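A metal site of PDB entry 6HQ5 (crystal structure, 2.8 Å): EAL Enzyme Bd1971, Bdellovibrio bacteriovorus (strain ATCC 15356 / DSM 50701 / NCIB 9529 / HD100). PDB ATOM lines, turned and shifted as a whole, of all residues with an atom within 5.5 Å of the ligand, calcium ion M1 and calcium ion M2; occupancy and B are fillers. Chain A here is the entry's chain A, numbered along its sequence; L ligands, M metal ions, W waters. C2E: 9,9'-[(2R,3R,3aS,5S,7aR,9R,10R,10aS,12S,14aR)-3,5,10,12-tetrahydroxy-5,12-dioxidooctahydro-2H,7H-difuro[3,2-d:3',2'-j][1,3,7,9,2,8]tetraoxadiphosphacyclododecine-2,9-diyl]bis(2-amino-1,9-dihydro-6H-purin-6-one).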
ATOM      1  N   LEU A 157     -12.000  29.624   3.656  1.00  0.00           N
ATOM      2  CA  LEU A 157     -12.381  28.455   2.836  1.00  0.00           C
ATOM      3  C   LEU A 157     -12.159  28.741   1.354  1.00  0.00           C
ATOM      4  O   LEU A 157     -12.605  29.763   0.841  1.00  0.00           O
ATOM      5  CB  LEU A 157     -13.847  28.055   3.058  1.00  0.00           C
ATOM      6  CG  LEU A 157     -14.290  27.629   4.463  1.00  0.00           C
ATOM      7  CD1 LEU A 157     -15.696  27.022   4.400  1.00  0.00           C
ATOM      8  CD2 LEU A 157     -13.317  26.633   5.085  1.00  0.00           C
ATOM      9  N   GLN A 160     -13.083  23.740  -4.484  1.00  0.00           N
ATOM     10  CA  GLN A 160     -12.637  23.046  -5.695  1.00  0.00           C
ATOM     11  C   GLN A 160     -13.808  22.427  -6.446  1.00  0.00           C
ATOM     12  O   GLN A 160     -14.536  21.621  -5.873  1.00  0.00           O
ATOM     13  CB  GLN A 160     -11.632  21.944  -5.373  1.00  0.00           C
ATOM     14  CG  GLN A 160     -11.122  21.264  -6.632  1.00  0.00           C
ATOM     15  CD  GLN A 160     -10.011  20.276  -6.357  1.00  0.00           C
ATOM     16  OE1 GLN A 160     -10.087  19.500  -5.407  1.00  0.00           O
ATOM     17  NE2 GLN A 160      -8.972  20.295  -7.191  1.00  0.00           N
ATOM     18  N   GLU A 174     -16.015  21.027  -3.389  1.00  0.00           N
ATOM     19  CA  GLU A 174     -15.566  20.649  -2.040  1.00  0.00           C
ATOM     20  C   GLU A 174     -14.986  21.874  -1.349  1.00  0.00           C
ATOM     21  O   GLU A 174     -14.209  22.618  -1.947  1.00  0.00           O
ATOM     22  CB  GLU A 174     -14.506  19.534  -2.088  1.00  0.00           C
ATOM     23  CG  GLU A 174     -14.125  19.005  -0.700  1.00  0.00           C
ATOM     24  CD  GLU A 174     -13.087  17.885  -0.711  1.00  0.00           C
ATOM     25  OE1 GLU A 174     -12.395  17.689  -1.735  1.00  0.00           O
ATOM     26  OE2 GLU A 174     -12.965  17.181   0.320  1.00  0.00           O
ATOM     27  N   ALA A 175     -15.374  22.067  -0.083  1.00  0.00           N
ATOM     28  CA  ALA A 175     -14.844  23.152   0.736  1.00  0.00           C
ATOM     29  C   ALA A 175     -13.546  22.706   1.405  1.00  0.00           C
ATOM     30  O   ALA A 175     -13.505  21.646   2.031  1.00  0.00           O
ATOM     31  CB  ALA A 175     -15.859  23.570   1.778  1.00  0.00           C
ATOM     32  N   LEU A 176     -12.498  23.515   1.281  1.00  0.00           N
ATOM     33  CA  LEU A 176     -11.191  23.186   1.844  1.00  0.00           C
ATOM     34  C   LEU A 176     -10.640  24.358   2.666  1.00  0.00           C
ATOM     35  O   LEU A 176     -10.666  25.508   2.226  1.00  0.00           O
ATOM     36  CB  LEU A 176     -10.214  22.827   0.725  1.00  0.00           C
ATOM     37  CG  LEU A 176     -10.633  21.614  -0.127  1.00  0.00           C
ATOM     38  CD1 LEU A 176      -9.763  21.508  -1.368  1.00  0.00           C
ATOM     39  CD2 LEU A 176     -10.574  20.339   0.696  1.00  0.00           C
ATOM     40  N   LEU A 177     -10.127  24.035   3.861  1.00  0.00           N
ATOM     41  CA  LEU A 177      -9.645  25.044   4.809  1.00  0.00           C
ATOM     42  C   LEU A 177      -8.275  25.558   4.411  1.00  0.00           C
ATOM     43  O   LEU A 177      -7.469  24.813   3.855  1.00  0.00           O
ATOM     44  CB  LEU A 177      -9.572  24.448   6.216  1.00  0.00           C
ATOM     45  CG  LEU A 177      -9.256  25.416   7.368  1.00  0.00           C
ATOM     46  CD1 LEU A 177     -10.423  26.380   7.584  1.00  0.00           C
ATOM     47  CD2 LEU A 177      -8.967  24.651   8.649  1.00  0.00           C
ATOM     48  N   ARG A 178      -8.020  26.825   4.700  1.00  0.00           N
ATOM     49  CA  ARG A 178      -6.733  27.463   4.381  1.00  0.00           C
ATOM     50  C   ARG A 178      -6.314  28.378   5.527  1.00  0.00           C
ATOM     51  O   ARG A 178      -7.146  29.112   6.079  1.00  0.00           O
ATOM     52  CB  ARG A 178      -6.847  28.273   3.080  1.00  0.00           C
ATOM     53  CG  ARG A 178      -7.020  27.435   1.819  1.00  0.00           C
ATOM     54  CD  ARG A 178      -5.717  26.790   1.424  1.00  0.00           C
ATOM     55  NE  ARG A 178      -5.804  26.027   0.185  1.00  0.00           N
ATOM     56  CZ  ARG A 178      -6.264  24.767   0.081  1.00  0.00           C
ATOM     57  NH1 ARG A 178      -6.692  24.097   1.147  1.00  0.00           N
ATOM     58  NH2 ARG A 178      -6.282  24.182  -1.104  1.00  0.00           N
ATOM     59  N   PRO A 189       1.363  21.153   5.955  1.00  0.00           N
ATOM     60  CA  PRO A 189       0.044  21.299   5.335  1.00  0.00           C
ATOM     61  C   PRO A 189      -1.065  20.500   6.025  1.00  0.00           C
ATOM     62  O   PRO A 189      -2.119  21.058   6.341  1.00  0.00           O
ATOM     63  CB  PRO A 189       0.250  20.760   3.918  1.00  0.00           C
ATOM     64  CG  PRO A 189       1.696  20.882   3.633  1.00  0.00           C
ATOM     65  CD  PRO A 189       2.424  21.041   4.940  1.00  0.00           C
ATOM     66  N   ILE A 193      -4.375  20.455  10.628  1.00  0.00           N
ATOM     67  CA  ILE A 193      -5.721  19.857  10.666  1.00  0.00           C
ATOM     68  C   ILE A 193      -5.735  18.712  11.692  1.00  0.00           C
ATOM     69  O   ILE A 193      -6.711  18.561  12.437  1.00  0.00           O
ATOM     70  CB  ILE A 193      -6.242  19.345   9.290  1.00  0.00           C
ATOM     71  CG1 ILE A 193      -6.206  20.414   8.189  1.00  0.00           C
ATOM     72  CG2 ILE A 193      -7.684  18.855   9.417  1.00  0.00           C
ATOM     73  CD1 ILE A 193      -4.900  20.534   7.432  1.00  0.00           C
ATOM     74  N   GLU A 197      -8.163  18.623  14.707  1.00  0.00           N
ATOM     75  CA  GLU A 197      -9.050  17.468  14.841  1.00  0.00           C
ATOM     76  C   GLU A 197      -8.931  16.694  16.163  1.00  0.00           C
ATOM     77  O   GLU A 197      -9.918  16.150  16.641  1.00  0.00           O
ATOM     78  CB  GLU A 197      -8.903  16.502  13.652  1.00  0.00           C
ATOM     79  CG  GLU A 197      -9.673  16.946  12.420  1.00  0.00           C
ATOM     80  CD  GLU A 197      -9.644  15.918  11.306  1.00  0.00           C
ATOM     81  OE1 GLU A 197      -8.814  14.981  11.358  1.00  0.00           O
ATOM     82  OE2 GLU A 197     -10.440  16.049  10.347  1.00  0.00           O
ATOM     83  N   ILE A 209     -16.690  26.597  10.093  1.00  0.00           N
ATOM     84  CA  ILE A 209     -16.507  26.053   8.742  1.00  0.00           C
ATOM     85  C   ILE A 209     -17.872  25.790   8.108  1.00  0.00           C
ATOM     86  O   ILE A 209     -18.161  26.289   7.012  1.00  0.00           O
ATOM     87  CB  ILE A 209     -15.663  24.768   8.750  1.00  0.00           C
ATOM     88  CG1 ILE A 209     -14.203  25.116   9.077  1.00  0.00           C
ATOM     89  CG2 ILE A 209     -15.737  24.056   7.410  1.00  0.00           C
ATOM     90  CD1 ILE A 209     -13.317  23.921   9.332  1.00  0.00           C
ATOM     91  N   ASN A 241     -16.049  18.765   4.777  1.00  0.00           N
ATOM     92  CA  ASN A 241     -15.268  17.745   5.472  1.00  0.00           C
ATOM     93  C   ASN A 241     -15.516  17.792   6.978  1.00  0.00           C
ATOM     94  O   ASN A 241     -15.039  18.689   7.662  1.00  0.00           O
ATOM     95  CB  ASN A 241     -13.776  17.930   5.173  1.00  0.00           C
ATOM     96  CG  ASN A 241     -13.400  17.487   3.771  1.00  0.00           C
ATOM     97  OD1 ASN A 241     -13.655  16.358   3.376  1.00  0.00           O
ATOM     98  ND2 ASN A 241     -12.779  18.387   3.015  1.00  0.00           N
ATOM     99  N   ILE A 242     -16.272  16.816   7.485  1.00  0.00           N
ATOM    100  CA  ILE A 242     -16.643  16.736   8.903  1.00  0.00           C
ATOM    101  C   ILE A 242     -15.756  15.707   9.618  1.00  0.00           C
ATOM    102  O   ILE A 242     -15.739  14.537   9.253  1.00  0.00           O
ATOM    103  CB  ILE A 242     -18.131  16.357   9.065  1.00  0.00           C
ATOM    104  CG1 ILE A 242     -19.031  17.596   8.941  1.00  0.00           C
ATOM    105  CG2 ILE A 242     -18.415  15.728  10.421  1.00  0.00           C
ATOM    106  CD1 ILE A 242     -18.841  18.398   7.675  1.00  0.00           C
ATOM    107  N   SER A 243     -15.035  16.160  10.638  1.00  0.00           N
ATOM    108  CA  SER A 243     -14.131  15.278  11.395  1.00  0.00           C
ATOM    109  C   SER A 243     -14.861  14.333  12.354  1.00  0.00           C
ATOM    110  O   SER A 243     -16.041  14.522  12.647  1.00  0.00           O
ATOM    111  CB  SER A 243     -13.120  16.101  12.195  1.00  0.00           C
ATOM    112  OG  SER A 243     -13.717  16.659  13.361  1.00  0.00           O
ATOM    113  N   GLN A 246     -16.103  15.952  15.899  1.00  0.00           N
ATOM    114  CA  GLN A 246     -17.208  16.901  15.752  1.00  0.00           C
ATOM    115  C   GLN A 246     -18.489  16.209  15.300  1.00  0.00           C
ATOM    116  O   GLN A 246     -19.585  16.722  15.529  1.00  0.00           O
ATOM    117  CB  GLN A 246     -16.843  18.066  14.810  1.00  0.00           C
ATOM    118  CG  GLN A 246     -16.924  17.782  13.311  1.00  0.00           C
ATOM    119  CD  GLN A 246     -16.546  19.003  12.474  1.00  0.00           C
ATOM    120  OE1 GLN A 246     -15.418  19.112  11.986  1.00  0.00           O
ATOM    121  NE2 GLN A 246     -17.485  19.936  12.299  1.00  0.00           N
ATOM    122  N   GLU A 273     -18.970  14.854   4.387  1.00  0.00           N
ATOM    123  CA  GLU A 273     -17.849  14.031   3.938  1.00  0.00           C
ATOM    124  C   GLU A 273     -16.969  13.557   5.105  1.00  0.00           C
ATOM    125  O   GLU A 273     -16.203  14.345   5.663  1.00  0.00           O
ATOM    126  CB  GLU A 273     -17.026  14.808   2.906  1.00  0.00           C
ATOM    127  CG  GLU A 273     -16.125  13.955   2.042  1.00  0.00           C
ATOM    128  CD  GLU A 273     -15.725  14.627   0.741  1.00  0.00           C
ATOM    129  OE1 GLU A 273     -16.616  15.150   0.026  1.00  0.00           O
ATOM    130  OE2 GLU A 273     -14.523  14.622   0.421  1.00  0.00           O
ATOM    131  N   ASP A 302     -14.696   9.529   2.229  1.00  0.00           N
ATOM    132  CA  ASP A 302     -13.461  10.024   1.657  1.00  0.00           C
ATOM    133  C   ASP A 302     -12.299   9.136   2.101  1.00  0.00           C
ATOM    134  O   ASP A 302     -12.367   8.502   3.159  1.00  0.00           O
ATOM    135  CB  ASP A 302     -13.232  11.471   2.115  1.00  0.00           C
ATOM    136  CG  ASP A 302     -12.056  12.152   1.410  1.00  0.00           C
ATOM    137  OD1 ASP A 302     -11.595  11.655   0.359  1.00  0.00           O
ATOM    138  OD2 ASP A 302     -11.614  13.197   1.924  1.00  0.00           O
ATOM    139  N   ASP A 303     -11.255   9.085   1.284  1.00  0.00           N
ATOM    140  CA  ASP A 303     -10.067   8.288   1.582  1.00  0.00           C
ATOM    141  C   ASP A 303     -10.450   6.826   1.793  1.00  0.00           C
ATOM    142  O   ASP A 303     -10.072   6.212   2.790  1.00  0.00           O
ATOM    143  CB  ASP A 303      -9.327   8.866   2.810  1.00  0.00           C
ATOM    144  CG  ASP A 303      -8.938  10.341   2.626  1.00  0.00           C
ATOM    145  OD1 ASP A 303      -8.558  10.739   1.499  1.00  0.00           O
ATOM    146  OD2 ASP A 303      -8.999  11.105   3.607  1.00  0.00           O
ATOM    147  N   LYS A 323     -15.308   8.348  -2.588  1.00  0.00           N
ATOM    148  CA  LYS A 323     -14.203   8.952  -3.331  1.00  0.00           C
ATOM    149  C   LYS A 323     -13.024   8.002  -3.526  1.00  0.00           C
ATOM    150  O   LYS A 323     -12.476   7.499  -2.553  1.00  0.00           O
ATOM    151  CB  LYS A 323     -13.705  10.206  -2.621  1.00  0.00           C
ATOM    152  CG  LYS A 323     -14.667  11.383  -2.656  1.00  0.00           C
ATOM    153  CD  LYS A 323     -13.919  12.708  -2.625  1.00  0.00           C
ATOM    154  CE  LYS A 323     -14.851  13.896  -2.762  1.00  0.00           C
ATOM    155  NZ  LYS A 323     -14.127  15.173  -2.529  1.00  0.00           N
ATOM    156  N   ASP A 325      -9.399   7.860  -3.822  1.00  0.00           N
ATOM    157  CA  ASP A 325      -8.417   8.813  -3.336  1.00  0.00           C
ATOM    158  C   ASP A 325      -7.314   9.097  -4.363  1.00  0.00           C
ATOM    159  O   ASP A 325      -7.068   8.298  -5.267  1.00  0.00           O
ATOM    160  CB  ASP A 325      -7.792   8.288  -2.038  1.00  0.00           C
ATOM    161  CG  ASP A 325      -7.032   9.350  -1.274  1.00  0.00           C
ATOM    162  OD1 ASP A 325      -7.668  10.339  -0.835  1.00  0.00           O
ATOM    163  OD2 ASP A 325      -5.797   9.198  -1.127  1.00  0.00           O
ATOM    164  N   ARG A 326      -6.678  10.261  -4.219  1.00  0.00           N
ATOM    165  CA  ARG A 326      -5.514  10.668  -5.024  1.00  0.00           C
ATOM    166  C   ARG A 326      -4.486   9.547  -5.172  1.00  0.00           C
ATOM    167  O   ARG A 326      -3.999   9.285  -6.268  1.00  0.00           O
ATOM    168  CB  ARG A 326      -4.802  11.853  -4.364  1.00  0.00           C
ATOM    169  CG  ARG A 326      -5.557  13.166  -4.368  1.00  0.00           C
ATOM    170  CD  ARG A 326      -4.746  14.251  -3.679  1.00  0.00           C
ATOM    171  NE  ARG A 326      -4.783  14.142  -2.219  1.00  0.00           N
ATOM    172  CZ  ARG A 326      -4.155  14.957  -1.377  1.00  0.00           C
ATOM    173  NH1 ARG A 326      -3.417  15.968  -1.839  1.00  0.00           N
ATOM    174  NH2 ARG A 326      -4.252  14.772  -0.068  1.00  0.00           N
ATOM    175  N   GLU A 359     -10.637  11.424  -7.609  1.00  0.00           N
ATOM    176  CA  GLU A 359      -9.940  12.525  -6.959  1.00  0.00           C
ATOM    177  C   GLU A 359      -8.511  12.600  -7.460  1.00  0.00           C
ATOM    178  O   GLU A 359      -7.871  11.579  -7.706  1.00  0.00           O
ATOM    179  CB  GLU A 359      -9.960  12.271  -5.457  1.00  0.00           C
ATOM    180  CG  GLU A 359      -9.558  13.417  -4.546  1.00  0.00           C
ATOM    181  CD  GLU A 359      -9.599  12.995  -3.087  1.00  0.00           C
ATOM    182  OE1 GLU A 359      -8.588  12.468  -2.555  1.00  0.00           O
ATOM    183  OE2 GLU A 359     -10.665  13.148  -2.481  1.00  0.00           O
ATOM    184  N   GLY A 360      -7.997  13.816  -7.615  1.00  0.00           N
ATOM    185  CA  GLY A 360      -6.597  14.027  -8.003  1.00  0.00           C
ATOM    186  C   GLY A 360      -6.278  13.785  -9.463  1.00  0.00           C
ATOM    187  O   GLY A 360      -5.176  13.340  -9.780  1.00  0.00           O
ATOM    188  N   ILE A 361      -7.211  14.095 -10.360  1.00  0.00           N
ATOM    189  CA  ILE A 361      -6.979  13.966 -11.799  1.00  0.00           C
ATOM    190  C   ILE A 361      -6.133  15.150 -12.293  1.00  0.00           C
ATOM    191  O   ILE A 361      -6.572  16.302 -12.200  1.00  0.00           O
ATOM    192  CB  ILE A 361      -8.300  13.935 -12.601  1.00  0.00           C
ATOM    193  CG1 ILE A 361      -9.181  12.761 -12.141  1.00  0.00           C
ATOM    194  CG2 ILE A 361      -8.024  13.806 -14.086  1.00  0.00           C
ATOM    195  CD1 ILE A 361     -10.636  12.902 -12.505  1.00  0.00           C
ATOM    196  N   GLU A 362      -4.952  14.859 -12.823  1.00  0.00           N
ATOM    197  CA  GLU A 362      -4.044  15.894 -13.337  1.00  0.00           C
ATOM    198  C   GLU A 362      -3.818  15.872 -14.856  1.00  0.00           C
ATOM    199  O   GLU A 362      -3.360  16.873 -15.414  1.00  0.00           O
ATOM    200  CB  GLU A 362      -2.696  15.798 -12.615  1.00  0.00           C
ATOM    201  CG  GLU A 362      -2.783  16.152 -11.141  1.00  0.00           C
ATOM    202  CD  GLU A 362      -1.451  16.078 -10.425  1.00  0.00           C
ATOM    203  OE1 GLU A 362      -0.444  15.686 -11.040  1.00  0.00           O
ATOM    204  OE2 GLU A 362      -1.423  16.434  -9.231  1.00  0.00           O
ATOM    205  N   GLN A 379     -12.564  15.268  -9.982  1.00  0.00           N
ATOM    206  CA  GLN A 379     -12.019  16.340  -9.153  1.00  0.00           C
ATOM    207  C   GLN A 379     -10.500  16.301  -9.312  1.00  0.00           C
ATOM    208  O   GLN A 379      -9.896  15.238  -9.210  1.00  0.00           O
ATOM    209  CB  GLN A 379     -12.430  16.111  -7.694  1.00  0.00           C
ATOM    210  CG  GLN A 379     -12.180  17.289  -6.764  1.00  0.00           C
ATOM    211  CD  GLN A 379     -12.622  17.014  -5.331  1.00  0.00           C
ATOM    212  OE1 GLN A 379     -13.336  16.046  -5.056  1.00  0.00           O
ATOM    213  NE2 GLN A 379     -12.191  17.866  -4.406  1.00  0.00           N
ATOM    214  N   GLY A 380      -9.884  17.440  -9.580  1.00  0.00           N
ATOM    215  CA  GLY A 380      -8.448  17.489  -9.818  1.00  0.00           C
ATOM    216  C   GLY A 380      -7.966  18.770 -10.480  1.00  0.00           C
ATOM    217  O   GLY A 380      -8.768  19.592 -10.919  1.00  0.00           O
ATOM    218  N   TYR A 381      -6.642  18.923 -10.541  1.00  0.00           N
ATOM    219  CA  TYR A 381      -6.027  20.113 -11.131  1.00  0.00           C
ATOM    220  C   TYR A 381      -6.258  20.203 -12.629  1.00  0.00           C
ATOM    221  O   TYR A 381      -6.276  21.300 -13.181  1.00  0.00           O
ATOM    222  CB  TYR A 381      -4.515  20.168 -10.843  1.00  0.00           C
ATOM    223  CG  TYR A 381      -4.115  20.379  -9.387  1.00  0.00           C
ATOM    224  CD1 TYR A 381      -5.031  20.841  -8.433  1.00  0.00           C
ATOM    225  CD2 TYR A 381      -2.804  20.152  -8.973  1.00  0.00           C
ATOM    226  CE1 TYR A 381      -4.646  21.029  -7.115  1.00  0.00           C
ATOM    227  CE2 TYR A 381      -2.419  20.340  -7.655  1.00  0.00           C
ATOM    228  CZ  TYR A 381      -3.341  20.781  -6.732  1.00  0.00           C
ATOM    229  OH  TYR A 381      -2.970  20.973  -5.428  1.00  0.00           O
ATOM    230  N   LEU A 382      -6.425  19.059 -13.296  1.00  0.00           N
ATOM    231  CA  LEU A 382      -6.771  19.045 -14.721  1.00  0.00           C
ATOM    232  C   LEU A 382      -7.903  20.029 -14.990  1.00  0.00           C
ATOM    233  O   LEU A 382      -7.824  20.844 -15.902  1.00  0.00           O
ATOM    234  CB  LEU A 382      -7.203  17.653 -15.173  1.00  0.00           C
ATOM    235  CG  LEU A 382      -7.578  17.512 -16.663  1.00  0.00           C
ATOM    236  CD1 LEU A 382      -6.332  17.614 -17.525  1.00  0.00           C
ATOM    237  CD2 LEU A 382      -8.307  16.214 -16.927  1.00  0.00           C
ATOM    238  N   PRO A 386      -8.338  24.231  -6.118  1.00  0.00           N
ATOM    239  CA  PRO A 386      -9.265  24.967  -5.263  1.00  0.00           C
ATOM    240  C   PRO A 386      -8.982  26.461  -5.302  1.00  0.00           C
ATOM    241  O   PRO A 386      -7.819  26.857  -5.359  1.00  0.00           O
ATOM    242  CB  PRO A 386      -9.008  24.390  -3.863  1.00  0.00           C
ATOM    243  CG  PRO A 386      -7.733  23.630  -3.969  1.00  0.00           C
ATOM    244  CD  PRO A 386      -7.605  23.180  -5.382  1.00  0.00           C
HETATM  245  P1  C2E L   1      -5.692  20.154   0.908  1.00  0.00           P
HETATM  246  O2P C2E L   1      -4.247  20.361   1.179  1.00  0.00           O
HETATM  247  O1P C2E L   1      -6.553  21.312   0.615  1.00  0.00           O
HETATM  248  O5' C2E L   1      -6.373  19.384   2.148  1.00  0.00           O
HETATM  249  C5' C2E L   1      -5.779  18.206   2.652  1.00  0.00           C
HETATM  250  C4' C2E L   1      -6.722  17.525   3.631  1.00  0.00           C
HETATM  251  O4' C2E L   1      -7.059  18.443   4.679  1.00  0.00           O
HETATM  252  C3' C2E L   1      -8.062  17.215   2.986  1.00  0.00           C
HETATM  253  O3' C2E L   1      -7.966  16.065   2.089  1.00  0.00           O
HETATM  254  C2' C2E L   1      -8.876  16.975   4.242  1.00  0.00           C
HETATM  255  O2' C2E L   1      -8.590  15.700   4.815  1.00  0.00           O
HETATM  256  C1' C2E L   1      -8.372  18.062   5.190  1.00  0.00           C
HETATM  257  N9  C2E L   1      -9.307  19.225   5.196  1.00  0.00           N
HETATM  258  C8  C2E L   1      -9.351  20.240   4.324  1.00  0.00           C
HETATM  259  N7  C2E L   1     -10.320  21.056   4.687  1.00  0.00           N
HETATM  260  C5  C2E L   1     -10.897  20.566   5.786  1.00  0.00           C
HETATM  261  C6  C2E L   1     -11.905  21.003   6.533  1.00  0.00           C
HETATM  262  O6  C2E L   1     -12.502  22.039   6.253  1.00  0.00           O
HETATM  263  N1  C2E L   1     -12.316  20.272   7.651  1.00  0.00           N
HETATM  264  C2  C2E L   1     -11.639  19.104   7.955  1.00  0.00           C
HETATM  265  N2  C2E L   1     -11.999  18.390   9.012  1.00  0.00           N
HETATM  266  N3  C2E L   1     -10.626  18.704   7.170  1.00  0.00           N
HETATM  267  C4  C2E L   1     -10.265  19.423   6.100  1.00  0.00           C
HETATM  268  P11 C2E L   1      -9.236  15.474   1.243  1.00  0.00           P
HETATM  269  O21 C2E L   1      -9.186  13.989   1.279  1.00  0.00           O
HETATM  270  O11 C2E L   1     -10.499  16.156   1.607  1.00  0.00           O
HETATM  271  O5A C2E L   1      -8.847  15.832  -0.302  1.00  0.00           O
HETATM  272  C5A C2E L   1      -8.698  17.149  -0.828  1.00  0.00           C
HETATM  273  C4A C2E L   1      -7.211  17.395  -1.118  1.00  0.00           C
HETATM  274  O4A C2E L   1      -6.829  16.929  -2.461  1.00  0.00           O
HETATM  275  C3A C2E L   1      -6.931  18.896  -1.094  1.00  0.00           C
HETATM  276  O3A C2E L   1      -5.737  19.117  -0.309  1.00  0.00           O
HETATM  277  C2A C2E L   1      -6.708  19.254  -2.541  1.00  0.00           C
HETATM  278  O2A C2E L   1      -5.806  20.390  -2.651  1.00  0.00           O
HETATM  279  C1A C2E L   1      -6.048  17.991  -3.071  1.00  0.00           C
HETATM  280  N91 C2E L   1      -6.093  17.892  -4.567  1.00  0.00           N
HETATM  281  C81 C2E L   1      -7.175  18.135  -5.300  1.00  0.00           C
HETATM  282  N71 C2E L   1      -6.873  17.950  -6.579  1.00  0.00           N
HETATM  283  C51 C2E L   1      -5.595  17.598  -6.655  1.00  0.00           C
HETATM  284  C61 C2E L   1      -4.823  17.301  -7.704  1.00  0.00           C
HETATM  285  O61 C2E L   1      -5.264  17.323  -8.857  1.00  0.00           O
HETATM  286  N11 C2E L   1      -3.489  16.946  -7.484  1.00  0.00           N
HETATM  287  C21 C2E L   1      -3.009  16.913  -6.184  1.00  0.00           C
HETATM  288  N21 C2E L   1      -1.749  16.576  -5.943  1.00  0.00           N
HETATM  289  N31 C2E L   1      -3.830  17.219  -5.169  1.00  0.00           N
HETATM  290  C41 C2E L   1      -5.112  17.561  -5.401  1.00  0.00           C
HETATM  291 CA    CA M   1     -12.643  15.261   1.590  1.00  0.00          CA
HETATM  292 CA    CA M   2      -8.821  12.262  -0.230  1.00  0.00          CA
HETATM  293  O   HOH W   1     -11.713  14.989  -0.511  1.00  0.00           O
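Residues that only touch the ligand: Leu 176, Ile 193, Ile 209, Gly 360, Ile 361, Gly 380 and Pro 386. Hydrophobic or aromatic side chains within 4 Å of the ligand: Leu 176, Leu 177, Ile 193, Ile 209, Tyr 381 and Pro 386. 19 residues have an atom within 4 Å of the ligand: Gln 160, Glu 174, Leu 176, Leu 177, Arg 178, Ile 193, Glu 197, Ile 209, Asn 241, Asp 302, Asp 303, Arg 326, Glu 359, Gly 360, Ile 361, Glu 362, Gly 380, Tyr 381 and Pro 386. The nearest printed residue that does not touch the ligand is Ser 243 (4.1 Å).
Calcium ion M2 is bound by OD1 of Asp 303, O21 of the ligand, OD1 of Asp 325, OE1 of Glu 359 and OD1 of Asp 302. Calcium ion M2 has five donor atoms within binding distance. Slightly farther from calcium ion M2 lies the side-chain carboxylate (OE2) of Glu 359 (3.0 Å).
The side-chain carboxylate of Glu 362 lies within hydrogen-bond range of a nitrogen (N11) of the ligand, 2.8 Å away. The side-chain carboxylate of Glu 197 lies within hydrogen-bond range of a nitrogen (N2) of the ligand (3.1 Å). The backbone NH (N) of Tyr 381 sits at hydrogen-bond distance from an oxygen (O61) of the ligand. NE2 of Gln 160 lies within hydrogen-bond range of N71 of the ligand (3.2 Å). The backbone NH (N) of Leu 177 lies within hydrogen-bond range of a nitrogen (N7) of the ligand (3.1 Å). O1P of the ligand is in salt-bridge range of NH1 of Arg 178. An oxygen (O4A) of the ligand lies within hydrogen-bond range of the guanidinium group (NE) of Arg 326 (3.5 Å). N1 of the ligand is in hydrogen-bond range of O of Asn 241 (3.1 Å).
O of Glu 273 is in hydrogen-bond range of N of Ile 242, 3.1 Å away. The backbone carbonyl oxygen of Ala 175 lies within hydrogen-bond range of the side-chain amide nitrogen of Asn 241, at 3.5 Å. The backbone carbonyl oxygen (O) of Gln 379 is in hydrogen-bond range of the backbone NH (N) of Ile 361 (3.1 Å). O of Ile 361 lies within hydrogen-bond range of N of Tyr 381, 3.1 Å away. The side-chain carboxylate (OE1) of Glu 359 lies close to the backbone NH (N) of Arg 326, at 3.4 Å. The backbone NH (N) of Leu 382 lies within hydrogen-bond range of the backbone carbonyl oxygen (O) of Ile 361 (3.0 Å). The backbone NH (N) of Gly 360 sits at hydrogen-bond distance from the backbone carbonyl oxygen (O) of Gln 379 (2.9 Å). OE1 of Glu 273 is in salt-bridge range of NZ of Lys 323.
Of the 30 residues printed, 4 come within 4 Å of calcium ion M1.
The side-chain carboxylate (OE2) of Glu 273 is bound to calcium ion M1 (2.3 Å). Water W1 binds calcium ion M1 (2.3 Å). Calcium ion M1 is bound by O11 of the ligand, at 2.3 Å. OE2 of Glu 174 binds calcium ion M1 (2.3 Å). Calcium ion M1 is bound by the side-chain amide oxygen (OD1) of Asn 241. Calcium ion M1 is bound by OD2 of Asp 302. Calcium ion M1 has six donor atoms within binding distance.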
